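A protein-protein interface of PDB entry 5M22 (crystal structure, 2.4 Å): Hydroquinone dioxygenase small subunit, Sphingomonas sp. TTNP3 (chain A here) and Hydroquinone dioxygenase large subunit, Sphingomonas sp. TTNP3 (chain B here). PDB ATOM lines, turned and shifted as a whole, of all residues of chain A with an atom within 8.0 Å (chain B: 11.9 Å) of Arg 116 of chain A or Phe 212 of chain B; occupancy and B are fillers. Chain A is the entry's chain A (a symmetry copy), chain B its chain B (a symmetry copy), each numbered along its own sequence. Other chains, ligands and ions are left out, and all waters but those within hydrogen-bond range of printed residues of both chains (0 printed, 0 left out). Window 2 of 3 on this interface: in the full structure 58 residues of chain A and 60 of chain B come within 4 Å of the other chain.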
ATOM      1  N   LEU A  88     -17.419 -33.369 -30.269  1.00  0.00           N
ATOM      2  CA  LEU A  88     -18.221 -32.170 -30.382  1.00  0.00           C
ATOM      3  C   LEU A  88     -18.115 -31.570 -31.761  1.00  0.00           C
ATOM      4  O   LEU A  88     -17.020 -31.434 -32.328  1.00  0.00           O
ATOM      5  CB  LEU A  88     -17.817 -31.142 -29.314  1.00  0.00           C
ATOM      6  CG  LEU A  88     -18.042 -31.552 -27.852  1.00  0.00           C
ATOM      7  CD1 LEU A  88     -17.174 -30.689 -26.943  1.00  0.00           C
ATOM      8  CD2 LEU A  88     -19.510 -31.499 -27.431  1.00  0.00           C
ATOM      9  N   LEU A  89     -19.293 -31.205 -32.258  1.00  0.00           N
ATOM     10  CA  LEU A  89     -19.507 -30.576 -33.554  1.00  0.00           C
ATOM     11  C   LEU A  89     -20.314 -29.280 -33.394  1.00  0.00           C
ATOM     12  O   LEU A  89     -21.409 -29.303 -32.820  1.00  0.00           O
ATOM     13  CB  LEU A  89     -20.313 -31.551 -34.409  1.00  0.00           C
ATOM     14  CG  LEU A  89     -20.471 -31.295 -35.888  1.00  0.00           C
ATOM     15  CD1 LEU A  89     -19.369 -32.037 -36.624  1.00  0.00           C
ATOM     16  CD2 LEU A  89     -21.818 -31.838 -36.290  1.00  0.00           C
ATOM     17  N   LYS A  90     -19.782 -28.163 -33.885  1.00  0.00           N
ATOM     18  CA  LYS A  90     -20.546 -26.913 -33.952  1.00  0.00           C
ATOM     19  C   LYS A  90     -21.511 -26.918 -35.165  1.00  0.00           C
ATOM     20  O   LYS A  90     -21.073 -26.899 -36.333  1.00  0.00           O
ATOM     21  CB  LYS A  90     -19.581 -25.707 -34.018  1.00  0.00           C
ATOM     22  CG  LYS A  90     -20.199 -24.317 -33.870  1.00  0.00           C
ATOM     23  CD  LYS A  90     -21.025 -24.179 -32.597  1.00  0.00           C
ATOM     24  CE  LYS A  90     -21.610 -22.778 -32.438  1.00  0.00           C
ATOM     25  NZ  LYS A  90     -20.840 -21.962 -31.429  1.00  0.00           N
ATOM     26  N   LEU A  91     -22.815 -26.938 -34.882  1.00  0.00           N
ATOM     27  CA  LEU A  91     -23.860 -27.031 -35.935  1.00  0.00           C
ATOM     28  C   LEU A  91     -24.013 -25.754 -36.765  1.00  0.00           C
ATOM     29  O   LEU A  91     -24.061 -24.649 -36.227  1.00  0.00           O
ATOM     30  CB  LEU A  91     -25.233 -27.388 -35.331  1.00  0.00           C
ATOM     31  CG  LEU A  91     -25.362 -28.721 -34.613  1.00  0.00           C
ATOM     32  CD1 LEU A  91     -26.803 -28.940 -34.186  1.00  0.00           C
ATOM     33  CD2 LEU A  91     -24.897 -29.837 -35.521  1.00  0.00           C
ATOM     34  N   ASP A  92     -24.117 -25.902 -38.075  1.00  0.00           N
ATOM     35  CA  ASP A  92     -24.247 -24.724 -38.908  1.00  0.00           C
ATOM     36  C   ASP A  92     -25.627 -24.139 -38.722  1.00  0.00           C
ATOM     37  O   ASP A  92     -25.781 -22.952 -38.737  1.00  0.00           O
ATOM     38  CB  ASP A  92     -24.004 -25.059 -40.374  1.00  0.00           C
ATOM     39  CG  ASP A  92     -22.592 -25.531 -40.641  1.00  0.00           C
ATOM     40  OD1 ASP A  92     -21.694 -25.273 -39.803  1.00  0.00           O
ATOM     41  OD2 ASP A  92     -22.386 -26.174 -41.696  1.00  0.00           O
ATOM     42  N   PRO A 113     -24.123 -34.864 -38.800  1.00  0.00           N
ATOM     43  CA  PRO A 113     -24.869 -33.635 -39.049  1.00  0.00           C
ATOM     44  C   PRO A 113     -23.910 -32.606 -39.601  1.00  0.00           C
ATOM     45  O   PRO A 113     -22.695 -32.782 -39.436  1.00  0.00           O
ATOM     46  CB  PRO A 113     -25.359 -33.217 -37.660  1.00  0.00           C
ATOM     47  CG  PRO A 113     -24.562 -34.011 -36.681  1.00  0.00           C
ATOM     48  CD  PRO A 113     -23.618 -34.926 -37.417  1.00  0.00           C
ATOM     49  N   GLU A 114     -24.439 -31.573 -40.257  1.00  0.00           N
ATOM     50  CA  GLU A 114     -23.616 -30.518 -40.855  1.00  0.00           C
ATOM     51  C   GLU A 114     -23.112 -29.519 -39.813  1.00  0.00           C
ATOM     52  O   GLU A 114     -23.877 -29.015 -38.992  1.00  0.00           O
ATOM     53  CB  GLU A 114     -24.392 -29.750 -41.955  1.00  0.00           C
ATOM     54  CG  GLU A 114     -24.673 -30.495 -43.255  1.00  0.00           C
ATOM     55  CD  GLU A 114     -23.459 -31.243 -43.804  1.00  0.00           C
ATOM     56  OE1 GLU A 114     -22.288 -30.808 -43.601  1.00  0.00           O
ATOM     57  OE2 GLU A 114     -23.689 -32.295 -44.442  1.00  0.00           O
ATOM     58  N   GLY A 115     -21.823 -29.220 -39.869  1.00  0.00           N
ATOM     59  CA  GLY A 115     -21.208 -28.261 -38.969  1.00  0.00           C
ATOM     60  C   GLY A 115     -19.725 -28.545 -38.975  1.00  0.00           C
ATOM     61  O   GLY A 115     -19.282 -29.403 -39.733  1.00  0.00           O
ATOM     62  N   ARG A 116     -18.967 -27.850 -38.121  1.00  0.00           N
ATOM     63  CA  ARG A 116     -17.513 -28.068 -38.020  1.00  0.00           C
ATOM     64  C   ARG A 116     -17.044 -28.581 -36.655  1.00  0.00           C
ATOM     65  O   ARG A 116     -17.749 -28.483 -35.625  1.00  0.00           O
ATOM     66  CB  ARG A 116     -16.705 -26.841 -38.469  1.00  0.00           C
ATOM     67  CG  ARG A 116     -16.955 -25.585 -37.666  1.00  0.00           C
ATOM     68  CD  ARG A 116     -16.651 -24.356 -38.499  1.00  0.00           C
ATOM     69  NE  ARG A 116     -16.371 -23.201 -37.638  1.00  0.00           N
ATOM     70  CZ  ARG A 116     -17.287 -22.485 -36.967  1.00  0.00           C
ATOM     71  NH1 ARG A 116     -16.886 -21.464 -36.220  1.00  0.00           N
ATOM     72  NH2 ARG A 116     -18.593 -22.768 -37.024  1.00  0.00           N
ATOM     73  N   LYS A 117     -15.832 -29.115 -36.674  1.00  0.00           N
ATOM     74  CA  LYS A 117     -15.306 -29.870 -35.581  1.00  0.00           C
ATOM     75  C   LYS A 117     -14.983 -28.926 -34.421  1.00  0.00           C
ATOM     76  O   LYS A 117     -14.160 -28.036 -34.580  1.00  0.00           O
ATOM     77  CB  LYS A 117     -14.060 -30.592 -36.075  1.00  0.00           C
ATOM     78  CG  LYS A 117     -13.805 -31.926 -35.422  1.00  0.00           C
ATOM     79  CD  LYS A 117     -12.383 -32.407 -35.694  1.00  0.00           C
ATOM     80  CE  LYS A 117     -11.827 -33.230 -34.526  1.00  0.00           C
ATOM     81  NZ  LYS A 117     -10.868 -34.287 -34.974  1.00  0.00           N
ATOM     82  N   MET A 118     -15.653 -29.102 -33.272  1.00  0.00           N
ATOM     83  CA  MET A 118     -15.343 -28.338 -32.033  1.00  0.00           C
ATOM     84  C   MET A 118     -14.153 -28.916 -31.245  1.00  0.00           C
ATOM     85  O   MET A 118     -13.248 -28.180 -30.848  1.00  0.00           O
ATOM     86  CB  MET A 118     -16.562 -28.247 -31.110  1.00  0.00           C
ATOM     87  CG  MET A 118     -17.610 -27.243 -31.532  1.00  0.00           C
ATOM     88  SD  MET A 118     -19.009 -27.158 -30.392  1.00  0.00           S
ATOM     89  CE  MET A 118     -18.362 -26.055 -29.143  1.00  0.00           C
ATOM     90  N   GLY A 119     -14.165 -30.233 -31.017  1.00  0.00           N
ATOM     91  CA  GLY A 119     -13.031 -30.910 -30.410  1.00  0.00           C
ATOM     92  C   GLY A 119     -13.394 -32.255 -29.831  1.00  0.00           C
ATOM     93  O   GLY A 119     -14.439 -32.829 -30.153  1.00  0.00           O
ATOM     94  N   PRO A 132     -22.326 -28.037 -24.429  1.00  0.00           N
ATOM     95  CA  PRO A 132     -22.879 -26.681 -24.585  1.00  0.00           C
ATOM     96  C   PRO A 132     -24.010 -26.664 -25.586  1.00  0.00           C
ATOM     97  O   PRO A 132     -23.902 -27.301 -26.634  1.00  0.00           O
ATOM     98  CB  PRO A 132     -21.691 -25.881 -25.109  1.00  0.00           C
ATOM     99  CG  PRO A 132     -20.868 -26.890 -25.847  1.00  0.00           C
ATOM    100  CD  PRO A 132     -21.038 -28.205 -25.125  1.00  0.00           C
ATOM    101  N   GLY A 134     -26.125 -25.812 -28.660  1.00  0.00           N
ATOM    102  CA  GLY A 134     -25.711 -25.467 -30.031  1.00  0.00           C
ATOM    103  C   GLY A 134     -24.641 -26.381 -30.626  1.00  0.00           C
ATOM    104  O   GLY A 134     -24.296 -26.267 -31.822  1.00  0.00           O
ATOM    105  N   ALA A 135     -24.085 -27.257 -29.786  1.00  0.00           N
ATOM    106  CA  ALA A 135     -23.189 -28.294 -30.231  1.00  0.00           C
ATOM    107  C   ALA A 135     -24.033 -29.534 -30.446  1.00  0.00           C
ATOM    108  O   ALA A 135     -25.067 -29.712 -29.792  1.00  0.00           O
ATOM    109  CB  ALA A 135     -22.124 -28.563 -29.180  1.00  0.00           C
ATOM    110  N   ALA A 136     -23.607 -30.392 -31.357  1.00  0.00           N
ATOM    111  CA  ALA A 136     -24.088 -31.758 -31.341  1.00  0.00           C
ATOM    112  C   ALA A 136     -22.990 -32.582 -30.658  1.00  0.00           C
ATOM    113  O   ALA A 136     -21.784 -32.252 -30.763  1.00  0.00           O
ATOM    114  CB  ALA A 136     -24.360 -32.258 -32.744  1.00  0.00           C
ATOM    115  N   ARG B 173     -21.435 -21.424 -14.437  1.00  0.00           N
ATOM    116  CA  ARG B 173     -21.752 -22.410 -15.465  1.00  0.00           C
ATOM    117  C   ARG B 173     -21.158 -23.814 -15.127  1.00  0.00           C
ATOM    118  O   ARG B 173     -21.897 -24.778 -14.865  1.00  0.00           O
ATOM    119  CB  ARG B 173     -21.273 -21.904 -16.833  1.00  0.00           C
ATOM    120  CG  ARG B 173     -22.128 -22.323 -18.025  1.00  0.00           C
ATOM    121  CD  ARG B 173     -21.554 -21.881 -19.381  1.00  0.00           C
ATOM    122  NE  ARG B 173     -22.176 -22.593 -20.519  1.00  0.00           N
ATOM    123  CZ  ARG B 173     -21.752 -22.557 -21.785  1.00  0.00           C
ATOM    124  NH1 ARG B 173     -20.708 -21.833 -22.147  1.00  0.00           N
ATOM    125  NH2 ARG B 173     -22.396 -23.235 -22.713  1.00  0.00           N
ATOM    126  N   MET B 174     -19.833 -23.926 -15.140  1.00  0.00           N
ATOM    127  CA  MET B 174     -19.154 -25.138 -14.721  1.00  0.00           C
ATOM    128  C   MET B 174     -17.778 -24.800 -14.205  1.00  0.00           C
ATOM    129  O   MET B 174     -17.134 -23.902 -14.692  1.00  0.00           O
ATOM    130  CB  MET B 174     -19.036 -26.126 -15.872  1.00  0.00           C
ATOM    131  CG  MET B 174     -18.675 -27.536 -15.443  1.00  0.00           C
ATOM    132  SD  MET B 174     -18.492 -28.577 -16.918  1.00  0.00           S
ATOM    133  CE  MET B 174     -16.761 -28.225 -17.302  1.00  0.00           C
ATOM    134  N   GLY B 176     -14.032 -24.572 -13.951  1.00  0.00           N
ATOM    135  CA  GLY B 176     -12.948 -24.611 -14.938  1.00  0.00           C
ATOM    136  C   GLY B 176     -13.110 -23.793 -16.214  1.00  0.00           C
ATOM    137  O   GLY B 176     -12.167 -23.689 -16.995  1.00  0.00           O
ATOM    138  N   LEU B 177     -14.297 -23.239 -16.451  1.00  0.00           N
ATOM    139  CA  LEU B 177     -14.545 -22.502 -17.691  1.00  0.00           C
ATOM    140  C   LEU B 177     -13.812 -21.180 -17.621  1.00  0.00           C
ATOM    141  O   LEU B 177     -13.485 -20.712 -16.516  1.00  0.00           O
ATOM    142  CB  LEU B 177     -16.049 -22.287 -17.944  1.00  0.00           C
ATOM    143  CG  LEU B 177     -16.757 -23.510 -18.540  1.00  0.00           C
ATOM    144  CD1 LEU B 177     -18.256 -23.505 -18.275  1.00  0.00           C
ATOM    145  CD2 LEU B 177     -16.474 -23.660 -20.024  1.00  0.00           C
ATOM    146  N   PRO B 178     -13.498 -20.587 -18.787  1.00  0.00           N
ATOM    147  CA  PRO B 178     -12.810 -19.287 -18.722  1.00  0.00           C
ATOM    148  C   PRO B 178     -13.623 -18.318 -17.871  1.00  0.00           C
ATOM    149  O   PRO B 178     -14.805 -18.095 -18.166  1.00  0.00           O
ATOM    150  CB  PRO B 178     -12.777 -18.826 -20.191  1.00  0.00           C
ATOM    151  CG  PRO B 178     -12.950 -20.073 -21.023  1.00  0.00           C
ATOM    152  CD  PRO B 178     -13.409 -21.205 -20.126  1.00  0.00           C
ATOM    153  N   VAL B 206      -8.537 -33.094 -22.758  1.00  0.00           N
ATOM    154  CA  VAL B 206      -9.381 -32.099 -23.440  1.00  0.00           C
ATOM    155  C   VAL B 206      -8.636 -31.592 -24.662  1.00  0.00           C
ATOM    156  O   VAL B 206      -7.483 -31.175 -24.556  1.00  0.00           O
ATOM    157  CB  VAL B 206      -9.776 -30.928 -22.511  1.00  0.00           C
ATOM    158  CG1 VAL B 206     -10.512 -29.837 -23.270  1.00  0.00           C
ATOM    159  CG2 VAL B 206     -10.646 -31.432 -21.375  1.00  0.00           C
ATOM    160  N   GLU B 207      -9.253 -31.688 -25.834  1.00  0.00           N
ATOM    161  CA  GLU B 207      -8.592 -31.200 -27.046  1.00  0.00           C
ATOM    162  C   GLU B 207      -9.541 -30.492 -28.005  1.00  0.00           C
ATOM    163  O   GLU B 207     -10.308 -31.107 -28.757  1.00  0.00           O
ATOM    164  CB  GLU B 207      -7.639 -32.230 -27.691  1.00  0.00           C
ATOM    165  CG  GLU B 207      -8.277 -33.465 -28.278  1.00  0.00           C
ATOM    166  CD  GLU B 207      -7.337 -34.664 -28.277  1.00  0.00           C
ATOM    167  OE1 GLU B 207      -6.606 -34.861 -27.291  1.00  0.00           O
ATOM    168  OE2 GLU B 207      -7.341 -35.424 -29.263  1.00  0.00           O
ATOM    169  N   ALA B 208      -9.471 -29.169 -27.889  1.00  0.00           N
ATOM    170  CA  ALA B 208     -10.279 -28.214 -28.624  1.00  0.00           C
ATOM    171  C   ALA B 208      -9.695 -27.924 -29.999  1.00  0.00           C
ATOM    172  O   ALA B 208      -8.473 -27.893 -30.160  1.00  0.00           O
ATOM    173  CB  ALA B 208     -10.379 -26.923 -27.830  1.00  0.00           C
ATOM    174  N   GLU B 209     -10.567 -27.713 -30.981  1.00  0.00           N
ATOM    175  CA  GLU B 209     -10.132 -27.251 -32.294  1.00  0.00           C
ATOM    176  C   GLU B 209      -9.928 -25.740 -32.220  1.00  0.00           C
ATOM    177  O   GLU B 209     -10.613 -25.059 -31.447  1.00  0.00           O
ATOM    178  CB  GLU B 209     -11.159 -27.595 -33.382  1.00  0.00           C
ATOM    179  CG  GLU B 209     -11.245 -29.063 -33.713  1.00  0.00           C
ATOM    180  CD  GLU B 209      -9.900 -29.620 -34.120  1.00  0.00           C
ATOM    181  OE1 GLU B 209      -9.355 -29.177 -35.161  1.00  0.00           O
ATOM    182  OE2 GLU B 209      -9.379 -30.486 -33.387  1.00  0.00           O
ATOM    183  N   PRO B 210      -8.987 -25.203 -33.014  1.00  0.00           N
ATOM    184  CA  PRO B 210      -8.812 -23.758 -33.005  1.00  0.00           C
ATOM    185  C   PRO B 210     -10.152 -22.997 -33.045  1.00  0.00           C
ATOM    186  O   PRO B 210     -11.000 -23.241 -33.921  1.00  0.00           O
ATOM    187  CB  PRO B 210      -7.995 -23.483 -34.283  1.00  0.00           C
ATOM    188  CG  PRO B 210      -7.776 -24.812 -34.949  1.00  0.00           C
ATOM    189  CD  PRO B 210      -8.029 -25.871 -33.919  1.00  0.00           C
ATOM    190  N   GLY B 211     -10.329 -22.081 -32.094  1.00  0.00           N
ATOM    191  CA  GLY B 211     -11.493 -21.217 -32.064  1.00  0.00           C
ATOM    192  C   GLY B 211     -12.518 -21.675 -31.067  1.00  0.00           C
ATOM    193  O   GLY B 211     -13.439 -20.949 -30.721  1.00  0.00           O
ATOM    194  N   PHE B 212     -12.362 -22.893 -30.590  1.00  0.00           N
ATOM    195  CA  PHE B 212     -13.355 -23.458 -29.719  1.00  0.00           C
ATOM    196  C   PHE B 212     -12.847 -23.714 -28.301  1.00  0.00           C
ATOM    197  O   PHE B 212     -13.604 -24.226 -27.481  1.00  0.00           O
ATOM    198  CB  PHE B 212     -13.901 -24.750 -30.343  1.00  0.00           C
ATOM    199  CG  PHE B 212     -14.717 -24.523 -31.590  1.00  0.00           C
ATOM    200  CD1 PHE B 212     -15.965 -23.885 -31.525  1.00  0.00           C
ATOM    201  CD2 PHE B 212     -14.247 -24.934 -32.836  1.00  0.00           C
ATOM    202  CE1 PHE B 212     -16.717 -23.677 -32.676  1.00  0.00           C
ATOM    203  CE2 PHE B 212     -14.996 -24.733 -33.991  1.00  0.00           C
ATOM    204  CZ  PHE B 212     -16.231 -24.106 -33.911  1.00  0.00           C
ATOM    205  N   GLU B 213     -11.599 -23.354 -27.995  1.00  0.00           N
ATOM    206  CA  GLU B 213     -11.023 -23.745 -26.705  1.00  0.00           C
ATOM    207  C   GLU B 213     -11.843 -23.279 -25.495  1.00  0.00           C
ATOM    208  O   GLU B 213     -11.710 -23.835 -24.412  1.00  0.00           O
ATOM    209  CB  GLU B 213      -9.510 -23.447 -26.588  1.00  0.00           C
ATOM    210  CG  GLU B 213      -9.042 -22.087 -27.055  1.00  0.00           C
ATOM    211  CD  GLU B 213      -9.029 -21.929 -28.573  1.00  0.00           C
ATOM    212  OE1 GLU B 213      -9.950 -21.267 -29.072  1.00  0.00           O
ATOM    213  OE2 GLU B 213      -8.108 -22.429 -29.258  1.00  0.00           O
ATOM    214  N   ALA B 214     -12.749 -22.332 -25.718  1.00  0.00           N
ATOM    215  CA  ALA B 214     -13.673 -21.850 -24.683  1.00  0.00           C
ATOM    216  C   ALA B 214     -14.892 -22.751 -24.432  1.00  0.00           C
ATOM    217  O   ALA B 214     -15.511 -22.676 -23.386  1.00  0.00           O
ATOM    218  CB  ALA B 214     -14.144 -20.423 -25.011  1.00  0.00           C
ATOM    219  N   GLU B 215     -15.271 -23.571 -25.394  1.00  0.00           N
ATOM    220  CA  GLU B 215     -16.527 -24.299 -25.267  1.00  0.00           C
ATOM    221  C   GLU B 215     -16.288 -25.782 -25.025  1.00  0.00           C
ATOM    222  O   GLU B 215     -17.229 -26.528 -24.717  1.00  0.00           O
ATOM    223  CB  GLU B 215     -17.413 -24.059 -26.503  1.00  0.00           C
ATOM    224  CG  GLU B 215     -17.995 -22.642 -26.581  1.00  0.00           C
ATOM    225  CD  GLU B 215     -19.329 -22.482 -25.835  1.00  0.00           C
ATOM    226  OE1 GLU B 215     -20.390 -22.775 -26.449  1.00  0.00           O
ATOM    227  OE2 GLU B 215     -19.330 -22.052 -24.654  1.00  0.00           O
ATOM    228  N   VAL B 216     -15.035 -26.195 -25.169  1.00  0.00           N
ATOM    229  CA  VAL B 216     -14.660 -27.600 -25.020  1.00  0.00           C
ATOM    230  C   VAL B 216     -14.010 -27.727 -23.646  1.00  0.00           C
ATOM    231  O   VAL B 216     -12.823 -27.387 -23.471  1.00  0.00           O
ATOM    232  CB  VAL B 216     -13.699 -28.051 -26.147  1.00  0.00           C
ATOM    233  CG1 VAL B 216     -13.274 -29.509 -25.990  1.00  0.00           C
ATOM    234  CG2 VAL B 216     -14.369 -27.883 -27.491  1.00  0.00           C
ATOM    235  N   SER B 217     -14.784 -28.187 -22.668  1.00  0.00           N
ATOM    236  CA  SER B 217     -14.342 -28.159 -21.268  1.00  0.00           C
ATOM    237  C   SER B 217     -14.666 -29.425 -20.470  1.00  0.00           C
ATOM    238  O   SER B 217     -15.810 -29.864 -20.424  1.00  0.00           O
ATOM    239  CB  SER B 217     -14.931 -26.945 -20.555  1.00  0.00           C
ATOM    240  OG  SER B 217     -14.267 -26.695 -19.344  1.00  0.00           O
ATOM    241  N   ALA B 218     -13.648 -30.005 -19.852  1.00  0.00           N
ATOM    242  CA  ALA B 218     -13.861 -31.007 -18.810  1.00  0.00           C
ATOM    243  C   ALA B 218     -12.890 -30.828 -17.642  1.00  0.00           C
ATOM    244  O   ALA B 218     -11.836 -30.196 -17.781  1.00  0.00           O
ATOM    245  CB  ALA B 218     -13.778 -32.410 -19.374  1.00  0.00           C
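Lys 90 of chain A touches Phe 212 of chain B (CB to CZ, 3.7 Å). CZ of Phe 212 of chain B touches NH1 of Arg 116 of chain A (3.6 Å). Lys 117 of chain A touches Glu 209 of chain B. Phe 212 of chain B touches Lys 117 of chain A (CE2 to O, 3.5 Å). Met 118 of chain A touches Ala 208 of chain B (O to C, 3.7 Å). O of Met 118 of chain A touches CB of Phe 212 of chain B (3.5 Å). O of Met 118 of chain A touches CG2 of Val 216 of chain B, 3.6 Å away. CA of Gly 119 of chain A touches O of Glu 207 of chain B, 3.2 Å away. Arg 173 of chain B touches Pro 132 of chain A. Glu 215 of chain B touches Pro 132 of chain A.
The backbone carbonyl oxygen of Met 118 of chain A sits at hydrogen-bond distance from the backbone NH of Glu 209 of chain B, 2.7 Å away.
No residue of chain B comes within 4 Å of Leu 89 of chain A. No residue of chain B comes within 4 Å of Gly 115 of chain A. Of the printed residues of chain B, Lys 117 of chain A touches Glu 209 and Phe 212. Met 118 of chain A touches just these residues of chain B: Ala 208 (3.7 Å), Glu 209 (2.7 Å), Phe 212 (3.5 Å), Glu 215 (3.4 Å) and Val 216 (3.6 Å). Gly 119 of chain A touches just one residue of chain B: Glu 207. Gly 176 of chain B touches none of the printed residues of chain A. Printed residues of chain A within 4 Å of Glu 207 of chain B: Gly 119. Printed residues of chain A within 4 Å of Glu 209 of chain B: Lys 117 (3.2 Å) and Met 118 (2.7 Å). Phe 212 of chain B touches just these residues of chain A: Lys 90 (3.7 Å), Arg 116 (3.6 Å), Lys 117 (3.5 Å) and Met 118 (3.5 Å). The nearest printed residue of chain B that does not touch Arg 116 of chain A is Gly 211 of chain B (6.5 Å).
Of the 18 printed residues of chain B, 7 touch a printed residue of chain A.
The backbone NH (N) of Met 118 of chain A sits at hydrogen-bond distance from the backbone carbonyl oxygen (O) of Leu 88 of chain A, at 2.9 Å. The backbone NH of Lys 90 of chain A lies close to the side-chain sulfur of Met 118 of chain A (3.7 Å). The backbone NH of Leu 88 of chain A lies within hydrogen-bond range of the backbone carbonyl oxygen of Gly 119 of chain A (3.0 Å). NH1 of Arg 173 of chain B is in salt-bridge range of OE2 of Glu 215 of chain B, 2.9 Å away. The backbone NH (N) of Lys 90 of chain A lies within hydrogen-bond range of the backbone carbonyl oxygen (O) of Arg 116 of chain A (2.7 Å).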
